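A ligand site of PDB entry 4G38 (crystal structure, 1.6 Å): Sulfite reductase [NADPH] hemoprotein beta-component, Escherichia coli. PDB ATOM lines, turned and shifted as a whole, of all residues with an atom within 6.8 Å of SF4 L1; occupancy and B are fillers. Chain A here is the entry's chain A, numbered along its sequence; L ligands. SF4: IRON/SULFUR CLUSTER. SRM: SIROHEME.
N of Cys 483 lies close to S2 of SF4 L1 (3.4 Å).
The side-chain sulfur (SG) of Cys 483 is bound to an iron atom (FE4) of SF4 L1 (2.2 Å).
An iron atom (FE2) of SF4 L1 is bound by the side-chain sulfur of Cys 440.
A sulfur (S4) of SF4 L1 sits close to the backbone NH (N) of Cys 479.
An iron atom (FE3) of SF4 L1 is bound by the side-chain sulfur (SG) of Cys 479 (2.3 Å).
The side-chain sulfur of Cys 434 is bound to an iron atom (FE1) of SF4 L1 (2.3 Å).
A sulfur (S2) of SF4 L1 sits close to the side-chain hydroxyl of Thr 477.
The side-chain amide nitrogen (ND2) of Asn 481 sits close to a sulfur (S1) of SF4 L1 (3.6 Å).
The backbone NH of Gly 482 sits close to a sulfur (S2) of SF4 L1, at 3.7 Å.
A sulfur (S3) of SF4 L1 sits close to the backbone NH of Ser 436, at 3.7 Å.
The side-chain sulfur of Cys 483 is bound to an iron atom (FE) of SRM L2, at 2.7 Å.
An oxygen (O1A) of SRM L2 is in hydrogen-bond range of the backbone NH of Cys 440 (3.4 Å).
O3B of SRM L2 sits at hydrogen-bond distance from N of Val 435 (3.1 Å).
Residues that only touch SF4 L1: Ala 443, Gly 478 and Leu 442.
Within 4 Å of SF4 L1: Cys 434, Ser 436, Cys 440, Leu 442, Ala 443, Thr 477, Gly 478, Cys 479, Asn 481, Gly 482 and Cys 483.
Along chain A the residues within 4 Å of SF4 L1 span positions 434 to 483.
The backbone NH (N) of Cys 483 sits at hydrogen-bond distance from the side-chain hydroxyl (OG1) of Thr 477.
The side-chain sulfur (SG) of Cys 440 lies close to the backbone NH (N) of Leu 442 (3.4 Å).
The side-chain amide nitrogen (ND2) of Asn 481 lies close to the side-chain sulfur (SG) of Cys 479, at 3.5 Å.
The side-chain sulfur (SG) of Cys 434 lies close to the backbone NH (N) of Gly 478.
The side-chain sulfur (SG) of Cys 434 lies close to the backbone NH (N) of Ser 436 (3.7 Å).
The side-chain hydroxyl (OG1) of Thr 477 sits at hydrogen-bond distance from the backbone NH (N) of Gly 484 (3.0 Å).
O of Gly 478 is in hydrogen-bond range of N of Met 444.
The backbone NH of Ala 445 sits at hydrogen-bond distance from the backbone carbonyl oxygen of Gly 478 (2.9 Å).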
ATOM      1  N   ALA A 433      -2.354 -16.697   8.051  1.00  0.00           N
ATOM      2  CA  ALA A 433      -2.382 -16.036   9.347  1.00  0.00           C
ATOM      3  C   ALA A 433      -1.825 -16.939  10.429  1.00  0.00           C
ATOM      4  O   ALA A 433      -1.820 -18.155  10.308  1.00  0.00           O
ATOM      5  CB  ALA A 433      -3.814 -15.662   9.701  1.00  0.00           C
ATOM      6  N   CYS A 434      -1.414 -16.333  11.539  1.00  0.00           N
ATOM      7  CA  CYS A 434      -1.018 -17.104  12.707  1.00  0.00           C
ATOM      8  C   CYS A 434      -2.240 -17.431  13.563  1.00  0.00           C
ATOM      9  O   CYS A 434      -3.348 -16.895  13.343  1.00  0.00           O
ATOM     10  CB  CYS A 434      -0.043 -16.312  13.572  1.00  0.00           C
ATOM     11  SG  CYS A 434      -0.843 -14.874  14.403  1.00  0.00           S
ATOM     12  N   VAL A 435      -2.022 -18.268  14.561  1.00  0.00           N
ATOM     13  CA  VAL A 435      -3.095 -18.675  15.475  1.00  0.00           C
ATOM     14  C   VAL A 435      -3.760 -17.487  16.197  1.00  0.00           C
ATOM     15  O   VAL A 435      -4.983 -17.329  16.144  1.00  0.00           O
ATOM     16  CB  VAL A 435      -2.561 -19.688  16.506  1.00  0.00           C
ATOM     17  CG1 VAL A 435      -3.611 -20.004  17.554  1.00  0.00           C
ATOM     18  CG2 VAL A 435      -2.108 -20.988  15.805  1.00  0.00           C
ATOM     19  N   SER A 436      -2.954 -16.661  16.866  1.00  0.00           N
ATOM     20  CA  SER A 436      -3.491 -15.501  17.590  1.00  0.00           C
ATOM     21  C   SER A 436      -4.574 -15.941  18.583  1.00  0.00           C
ATOM     22  O   SER A 436      -4.482 -17.021  19.171  1.00  0.00           O
ATOM     23  CB  SER A 436      -4.026 -14.453  16.596  1.00  0.00           C
ATOM     24  OG  SER A 436      -4.393 -13.253  17.270  1.00  0.00           O
ATOM     25  N   PHE A 437      -5.583 -15.091  18.787  1.00  0.00           N
ATOM     26  CA  PHE A 437      -6.698 -15.448  19.656  1.00  0.00           C
ATOM     27  C   PHE A 437      -7.399 -16.668  19.059  1.00  0.00           C
ATOM     28  O   PHE A 437      -7.481 -16.801  17.832  1.00  0.00           O
ATOM     29  CB  PHE A 437      -7.716 -14.294  19.778  1.00  0.00           C
ATOM     30  CG  PHE A 437      -7.139 -13.011  20.353  1.00  0.00           C
ATOM     31  CD1 PHE A 437      -6.860 -12.911  21.707  1.00  0.00           C
ATOM     32  CD2 PHE A 437      -6.954 -11.898  19.551  1.00  0.00           C
ATOM     33  CE1 PHE A 437      -6.378 -11.726  22.254  1.00  0.00           C
ATOM     34  CE2 PHE A 437      -6.450 -10.712  20.086  1.00  0.00           C
ATOM     35  CZ  PHE A 437      -6.173 -10.633  21.441  1.00  0.00           C
ATOM     36  N   CYS A 440      -3.508 -17.814  21.926  1.00  0.00           N
ATOM     37  CA  CYS A 440      -2.201 -17.190  22.103  1.00  0.00           C
ATOM     38  C   CYS A 440      -2.228 -16.114  23.192  1.00  0.00           C
ATOM     39  O   CYS A 440      -2.972 -15.154  23.074  1.00  0.00           O
ATOM     40  CB  CYS A 440      -1.697 -16.561  20.807  1.00  0.00           C
ATOM     41  SG  CYS A 440      -0.024 -15.958  21.031  1.00  0.00           S
ATOM     42  N   PRO A 441      -1.412 -16.284  24.239  1.00  0.00           N
ATOM     43  CA  PRO A 441      -1.402 -15.285  25.306  1.00  0.00           C
ATOM     44  C   PRO A 441      -0.769 -13.955  24.903  1.00  0.00           C
ATOM     45  O   PRO A 441      -0.893 -12.960  25.624  1.00  0.00           O
ATOM     46  CB  PRO A 441      -0.580 -15.968  26.422  1.00  0.00           C
ATOM     47  CG  PRO A 441       0.325 -16.911  25.693  1.00  0.00           C
ATOM     48  CD  PRO A 441      -0.472 -17.397  24.498  1.00  0.00           C
ATOM     49  N   LEU A 442      -0.092 -13.918  23.758  1.00  0.00           N
ATOM     50  CA  LEU A 442       0.632 -12.717  23.357  1.00  0.00           C
ATOM     51  C   LEU A 442      -0.146 -11.869  22.330  1.00  0.00           C
ATOM     52  O   LEU A 442       0.283 -10.775  21.977  1.00  0.00           O
ATOM     53  CB  LEU A 442       2.008 -13.102  22.760  1.00  0.00           C
ATOM     54  CG  LEU A 442       2.795 -14.145  23.566  1.00  0.00           C
ATOM     55  CD1 LEU A 442       4.167 -14.467  22.954  1.00  0.00           C
ATOM     56  CD2 LEU A 442       2.955 -13.729  25.024  1.00  0.00           C
ATOM     57  N   ALA A 443      -1.272 -12.383  21.849  1.00  0.00           N
ATOM     58  CA  ALA A 443      -2.019 -11.759  20.751  1.00  0.00           C
ATOM     59  C   ALA A 443      -2.428 -10.316  21.038  1.00  0.00           C
ATOM     60  O   ALA A 443      -2.815  -9.978  22.170  1.00  0.00           O
ATOM     61  CB  ALA A 443      -3.265 -12.603  20.419  1.00  0.00           C
ATOM     62  N   MET A 444      -2.340  -9.484  20.003  1.00  0.00           N
ATOM     63  CA  MET A 444      -2.850  -8.102  20.051  1.00  0.00           C
ATOM     64  C   MET A 444      -4.086  -7.906  19.185  1.00  0.00           C
ATOM     65  O   MET A 444      -5.004  -7.196  19.587  1.00  0.00           O
ATOM     66  CB  MET A 444      -1.766  -7.117  19.628  1.00  0.00           C
ATOM     67  CG  MET A 444      -0.588  -7.149  20.577  1.00  0.00           C
ATOM     68  SD  MET A 444       0.728  -6.076  20.020  1.00  0.00           S
ATOM     69  CE  MET A 444       1.995  -6.427  21.241  1.00  0.00           C
ATOM     70  N   ALA A 445      -4.086  -8.519  17.999  1.00  0.00           N
ATOM     71  CA  ALA A 445      -5.255  -8.508  17.134  1.00  0.00           C
ATOM     72  C   ALA A 445      -5.522  -9.916  16.597  1.00  0.00           C
ATOM     73  O   ALA A 445      -4.603 -10.723  16.502  1.00  0.00           O
ATOM     74  CB  ALA A 445      -5.073  -7.541  15.975  1.00  0.00           C
ATOM     75  N   ALA A 447      -6.022 -12.937  14.086  1.00  0.00           N
ATOM     76  CA  ALA A 447      -5.342 -13.277  12.844  1.00  0.00           C
ATOM     77  C   ALA A 447      -6.075 -14.454  12.195  1.00  0.00           C
ATOM     78  O   ALA A 447      -6.838 -14.247  11.258  1.00  0.00           O
ATOM     79  CB  ALA A 447      -3.868 -13.588  13.089  1.00  0.00           C
ATOM     80  N   VAL A 476      -1.323 -12.168   7.692  1.00  0.00           N
ATOM     81  CA  VAL A 476      -1.760 -11.437   8.896  1.00  0.00           C
ATOM     82  C   VAL A 476      -1.127 -12.083  10.108  1.00  0.00           C
ATOM     83  O   VAL A 476      -1.267 -13.274  10.326  1.00  0.00           O
ATOM     84  CB  VAL A 476      -3.280 -11.463   9.056  1.00  0.00           C
ATOM     85  CG1 VAL A 476      -3.715 -10.647  10.303  1.00  0.00           C
ATOM     86  CG2 VAL A 476      -3.976 -10.962   7.765  1.00  0.00           C
ATOM     87  N   THR A 477      -0.419 -11.301  10.916  1.00  0.00           N
ATOM     88  CA  THR A 477       0.181 -11.823  12.131  1.00  0.00           C
ATOM     89  C   THR A 477      -0.427 -11.028  13.286  1.00  0.00           C
ATOM     90  O   THR A 477      -0.677  -9.817  13.149  1.00  0.00           O
ATOM     91  CB  THR A 477       1.736 -11.786  12.037  1.00  0.00           C
ATOM     92  OG1 THR A 477       2.327 -12.688  12.992  1.00  0.00           O
ATOM     93  CG2 THR A 477       2.283 -10.365  12.231  1.00  0.00           C
ATOM     94  N   GLY A 478      -0.742 -11.711  14.380  1.00  0.00           N
ATOM     95  CA  GLY A 478      -1.519 -11.129  15.457  1.00  0.00           C
ATOM     96  C   GLY A 478      -0.793 -10.184  16.401  1.00  0.00           C
ATOM     97  O   GLY A 478      -1.424  -9.451  17.158  1.00  0.00           O
ATOM     98  N   CYS A 479       0.536 -10.235  16.383  1.00  0.00           N
ATOM     99  CA  CYS A 479       1.361  -9.305  17.130  1.00  0.00           C
ATOM    100  C   CYS A 479       2.718  -9.283  16.423  1.00  0.00           C
ATOM    101  O   CYS A 479       2.910 -10.004  15.432  1.00  0.00           O
ATOM    102  CB  CYS A 479       1.468  -9.730  18.609  1.00  0.00           C
ATOM    103  SG  CYS A 479       2.671 -11.035  18.920  1.00  0.00           S
ATOM    104  N   PRO A 480       3.657  -8.443  16.892  1.00  0.00           N
ATOM    105  CA  PRO A 480       4.873  -8.260  16.089  1.00  0.00           C
ATOM    106  C   PRO A 480       5.875  -9.397  16.225  1.00  0.00           C
ATOM    107  O   PRO A 480       6.888  -9.349  15.540  1.00  0.00           O
ATOM    108  CB  PRO A 480       5.455  -6.948  16.634  1.00  0.00           C
ATOM    109  CG  PRO A 480       4.961  -6.862  18.044  1.00  0.00           C
ATOM    110  CD  PRO A 480       3.595  -7.509  18.030  1.00  0.00           C
ATOM    111  N   ASN A 481       5.606 -10.388  17.054  1.00  0.00           N
ATOM    112  CA  ASN A 481       6.464 -11.567  17.089  1.00  0.00           C
ATOM    113  C   ASN A 481       6.575 -12.187  15.703  1.00  0.00           C
ATOM    114  O   ASN A 481       7.598 -12.762  15.354  1.00  0.00           O
ATOM    115  CB  ASN A 481       5.961 -12.573  18.113  1.00  0.00           C
ATOM    116  CG  ASN A 481       6.297 -12.167  19.517  1.00  0.00           C
ATOM    117  OD1 ASN A 481       7.342 -11.546  19.786  1.00  0.00           O
ATOM    118  ND2 ASN A 481       5.417 -12.515  20.454  1.00  0.00           N
ATOM    119  N   GLY A 482       5.505 -12.078  14.925  1.00  0.00           N
ATOM    120  CA  GLY A 482       5.599 -12.300  13.492  1.00  0.00           C
ATOM    121  C   GLY A 482       5.392 -13.704  12.956  1.00  0.00           C
ATOM    122  O   GLY A 482       5.801 -14.009  11.827  1.00  0.00           O
ATOM    123  N   CYS A 483       4.762 -14.556  13.759  1.00  0.00           N
ATOM    124  CA  CYS A 483       4.544 -15.965  13.425  1.00  0.00           C
ATOM    125  C   CYS A 483       3.851 -16.197  12.091  1.00  0.00           C
ATOM    126  O   CYS A 483       4.111 -17.196  11.416  1.00  0.00           O
ATOM    127  CB  CYS A 483       3.725 -16.639  14.518  1.00  0.00           C
ATOM    128  SG  CYS A 483       4.386 -16.378  16.184  1.00  0.00           S
ATOM    129  N   GLY A 484       2.948 -15.290  11.714  1.00  0.00           N
ATOM    130  CA  GLY A 484       2.254 -15.436  10.445  1.00  0.00           C
ATOM    131  C   GLY A 484       3.131 -15.095   9.243  1.00  0.00           C
ATOM    132  O   GLY A 484       2.686 -15.232   8.101  1.00  0.00           O
HETATM  133 FE1  SF4 L   1       0.385 -14.554  16.372  1.00  0.00          FE
HETATM  134 FE2  SF4 L   1       0.629 -15.228  18.964  1.00  0.00          FE
HETATM  135 FE3  SF4 L   1       1.835 -12.991  18.050  1.00  0.00          FE
HETATM  136 FE4  SF4 L   1       2.655 -15.422  17.196  1.00  0.00          FE
HETATM  137  S1  SF4 L   1       2.783 -14.645  19.206  1.00  0.00           S
HETATM  138  S2  SF4 L   1       2.322 -13.566  15.988  1.00  0.00           S
HETATM  139  S3  SF4 L   1       0.756 -16.544  17.231  1.00  0.00           S
HETATM  140  S4  SF4 L   1      -0.349 -13.432  18.095  1.00  0.00           S
HETATM  141 FE   SRM L   2       5.673 -18.639  16.958  1.00  0.00          FE
HETATM  142  CHA SRM L   2       5.655 -17.524  20.209  1.00  0.00           C
HETATM  143  CHB SRM L   2       2.552 -19.846  17.335  1.00  0.00           C
HETATM  144  CHC SRM L   2       5.761 -19.899  13.812  1.00  0.00           C
HETATM  145  CHD SRM L   2       7.975 -16.303  16.143  1.00  0.00           C
HETATM  146  NA  SRM L   2       4.407 -18.728  18.488  1.00  0.00           N
HETATM  147  C1A SRM L   2       4.593 -18.313  19.796  1.00  0.00           C
HETATM  148  C2A SRM L   2       3.554 -18.909  20.734  1.00  0.00           C
HETATM  149  CMA SRM L   2       4.053 -20.231  21.307  1.00  0.00           C
HETATM  150  CDA SRM L   2       3.126 -17.921  21.840  1.00  0.00           C
HETATM  151  CEA SRM L   2       3.832 -18.063  23.181  1.00  0.00           C
HETATM  152  O3A SRM L   2       5.055 -17.832  23.313  1.00  0.00           O
HETATM  153  O4A SRM L   2       3.196 -18.402  24.209  1.00  0.00           O
HETATM  154  C3A SRM L   2       2.441 -19.123  19.764  1.00  0.00           C
HETATM  155  CAA SRM L   2       1.347 -20.064  20.218  1.00  0.00           C
HETATM  156  CBA SRM L   2      -0.003 -19.652  19.624  1.00  0.00           C
HETATM  157  CCA SRM L   2      -1.015 -20.757  19.866  1.00  0.00           C
HETATM  158  O1A SRM L   2      -1.913 -20.628  20.732  1.00  0.00           O
HETATM  159  O2A SRM L   2      -0.954 -21.818  19.218  1.00  0.00           O
HETATM  160  C4A SRM L   2       3.147 -19.224  18.435  1.00  0.00           C
HETATM  161  NB  SRM L   2       4.454 -19.706  15.836  1.00  0.00           N
HETATM  162  C1B SRM L   2       3.174 -20.105  16.134  1.00  0.00           C
HETATM  163  C2B SRM L   2       2.563 -20.874  14.982  1.00  0.00           C
HETATM  164  CMB SRM L   2       1.633 -21.996  15.487  1.00  0.00           C
HETATM  165  CDB SRM L   2       1.772 -19.950  14.037  1.00  0.00           C
HETATM  166  CEB SRM L   2       0.892 -20.646  13.002  1.00  0.00           C
HETATM  167  O3B SRM L   2      -0.286 -20.260  12.870  1.00  0.00           O
HETATM  168  O4B SRM L   2       1.304 -21.575  12.282  1.00  0.00           O
HETATM  169  C3B SRM L   2       3.818 -21.416  14.369  1.00  0.00           C
HETATM  170  CAB SRM L   2       4.222 -22.750  14.979  1.00  0.00           C
HETATM  171  CBB SRM L   2       5.496 -23.200  14.251  1.00  0.00           C
HETATM  172  CCB SRM L   2       6.082 -24.422  14.931  1.00  0.00           C
HETATM  173  O1B SRM L   2       5.578 -25.550  14.724  1.00  0.00           O
HETATM  174  O2B SRM L   2       7.068 -24.318  15.691  1.00  0.00           O
HETATM  175  C4B SRM L   2       4.729 -20.280  14.642  1.00  0.00           C
HETATM  176  NC  SRM L   2       6.683 -18.205  15.318  1.00  0.00           N
HETATM  177  C1C SRM L   2       6.573 -18.829  14.109  1.00  0.00           C
HETATM  178  C2C SRM L   2       7.433 -18.194  13.077  1.00  0.00           C
HETATM  179  CDC SRM L   2       7.379 -18.435  11.600  1.00  0.00           C
HETATM  180  CEC SRM L   2       8.354 -19.527  11.260  1.00  0.00           C
HETATM  181  O3C SRM L   2       9.158 -20.006  12.108  1.00  0.00           O
HETATM  182  O4C SRM L   2       8.380 -19.991  10.113  1.00  0.00           O
HETATM  183  C3C SRM L   2       8.005 -17.023  13.719  1.00  0.00           C
HETATM  184  CAC SRM L   2       8.639 -15.868  12.989  1.00  0.00           C
HETATM  185  CBC SRM L   2      10.064 -16.215  12.524  1.00  0.00           C
HETATM  186  CCC SRM L   2      11.048 -15.926  13.629  1.00  0.00           C
HETATM  187  O1C SRM L   2      11.182 -16.752  14.568  1.00  0.00           O
HETATM  188  O2C SRM L   2      11.748 -14.875  13.636  1.00  0.00           O
HETATM  189  C4C SRM L   2       7.554 -17.160  15.140  1.00  0.00           C
HETATM  190  ND  SRM L   2       6.747 -17.327  18.003  1.00  0.00           N
HETATM  191  C1D SRM L   2       7.587 -16.403  17.462  1.00  0.00           C
HETATM  192  C2D SRM L   2       8.160 -15.493  18.489  1.00  0.00           C
HETATM  193  CAD SRM L   2       9.202 -14.406  18.342  1.00  0.00           C
HETATM  194  CBD SRM L   2      10.569 -15.001  18.638  1.00  0.00           C
HETATM  195  CCD SRM L   2      11.625 -13.933  18.539  1.00  0.00           C
HETATM  196  O1D SRM L   2      12.650 -14.153  17.843  1.00  0.00           O
HETATM  197  O2D SRM L   2      11.494 -12.828  19.109  1.00  0.00           O
HETATM  198  C3D SRM L   2       7.423 -15.835  19.701  1.00  0.00           C
HETATM  199  CDD SRM L   2       7.486 -15.135  21.026  1.00  0.00           C
HETATM  200  CED SRM L   2       8.560 -15.679  21.942  1.00  0.00           C
HETATM  201  O3D SRM L   2       9.190 -16.725  21.659  1.00  0.00           O
HETATM  202  O4D SRM L   2       8.823 -15.087  23.016  1.00  0.00           O
HETATM  203  C4D SRM L   2       6.565 -16.982  19.308  1.00  0.00           C
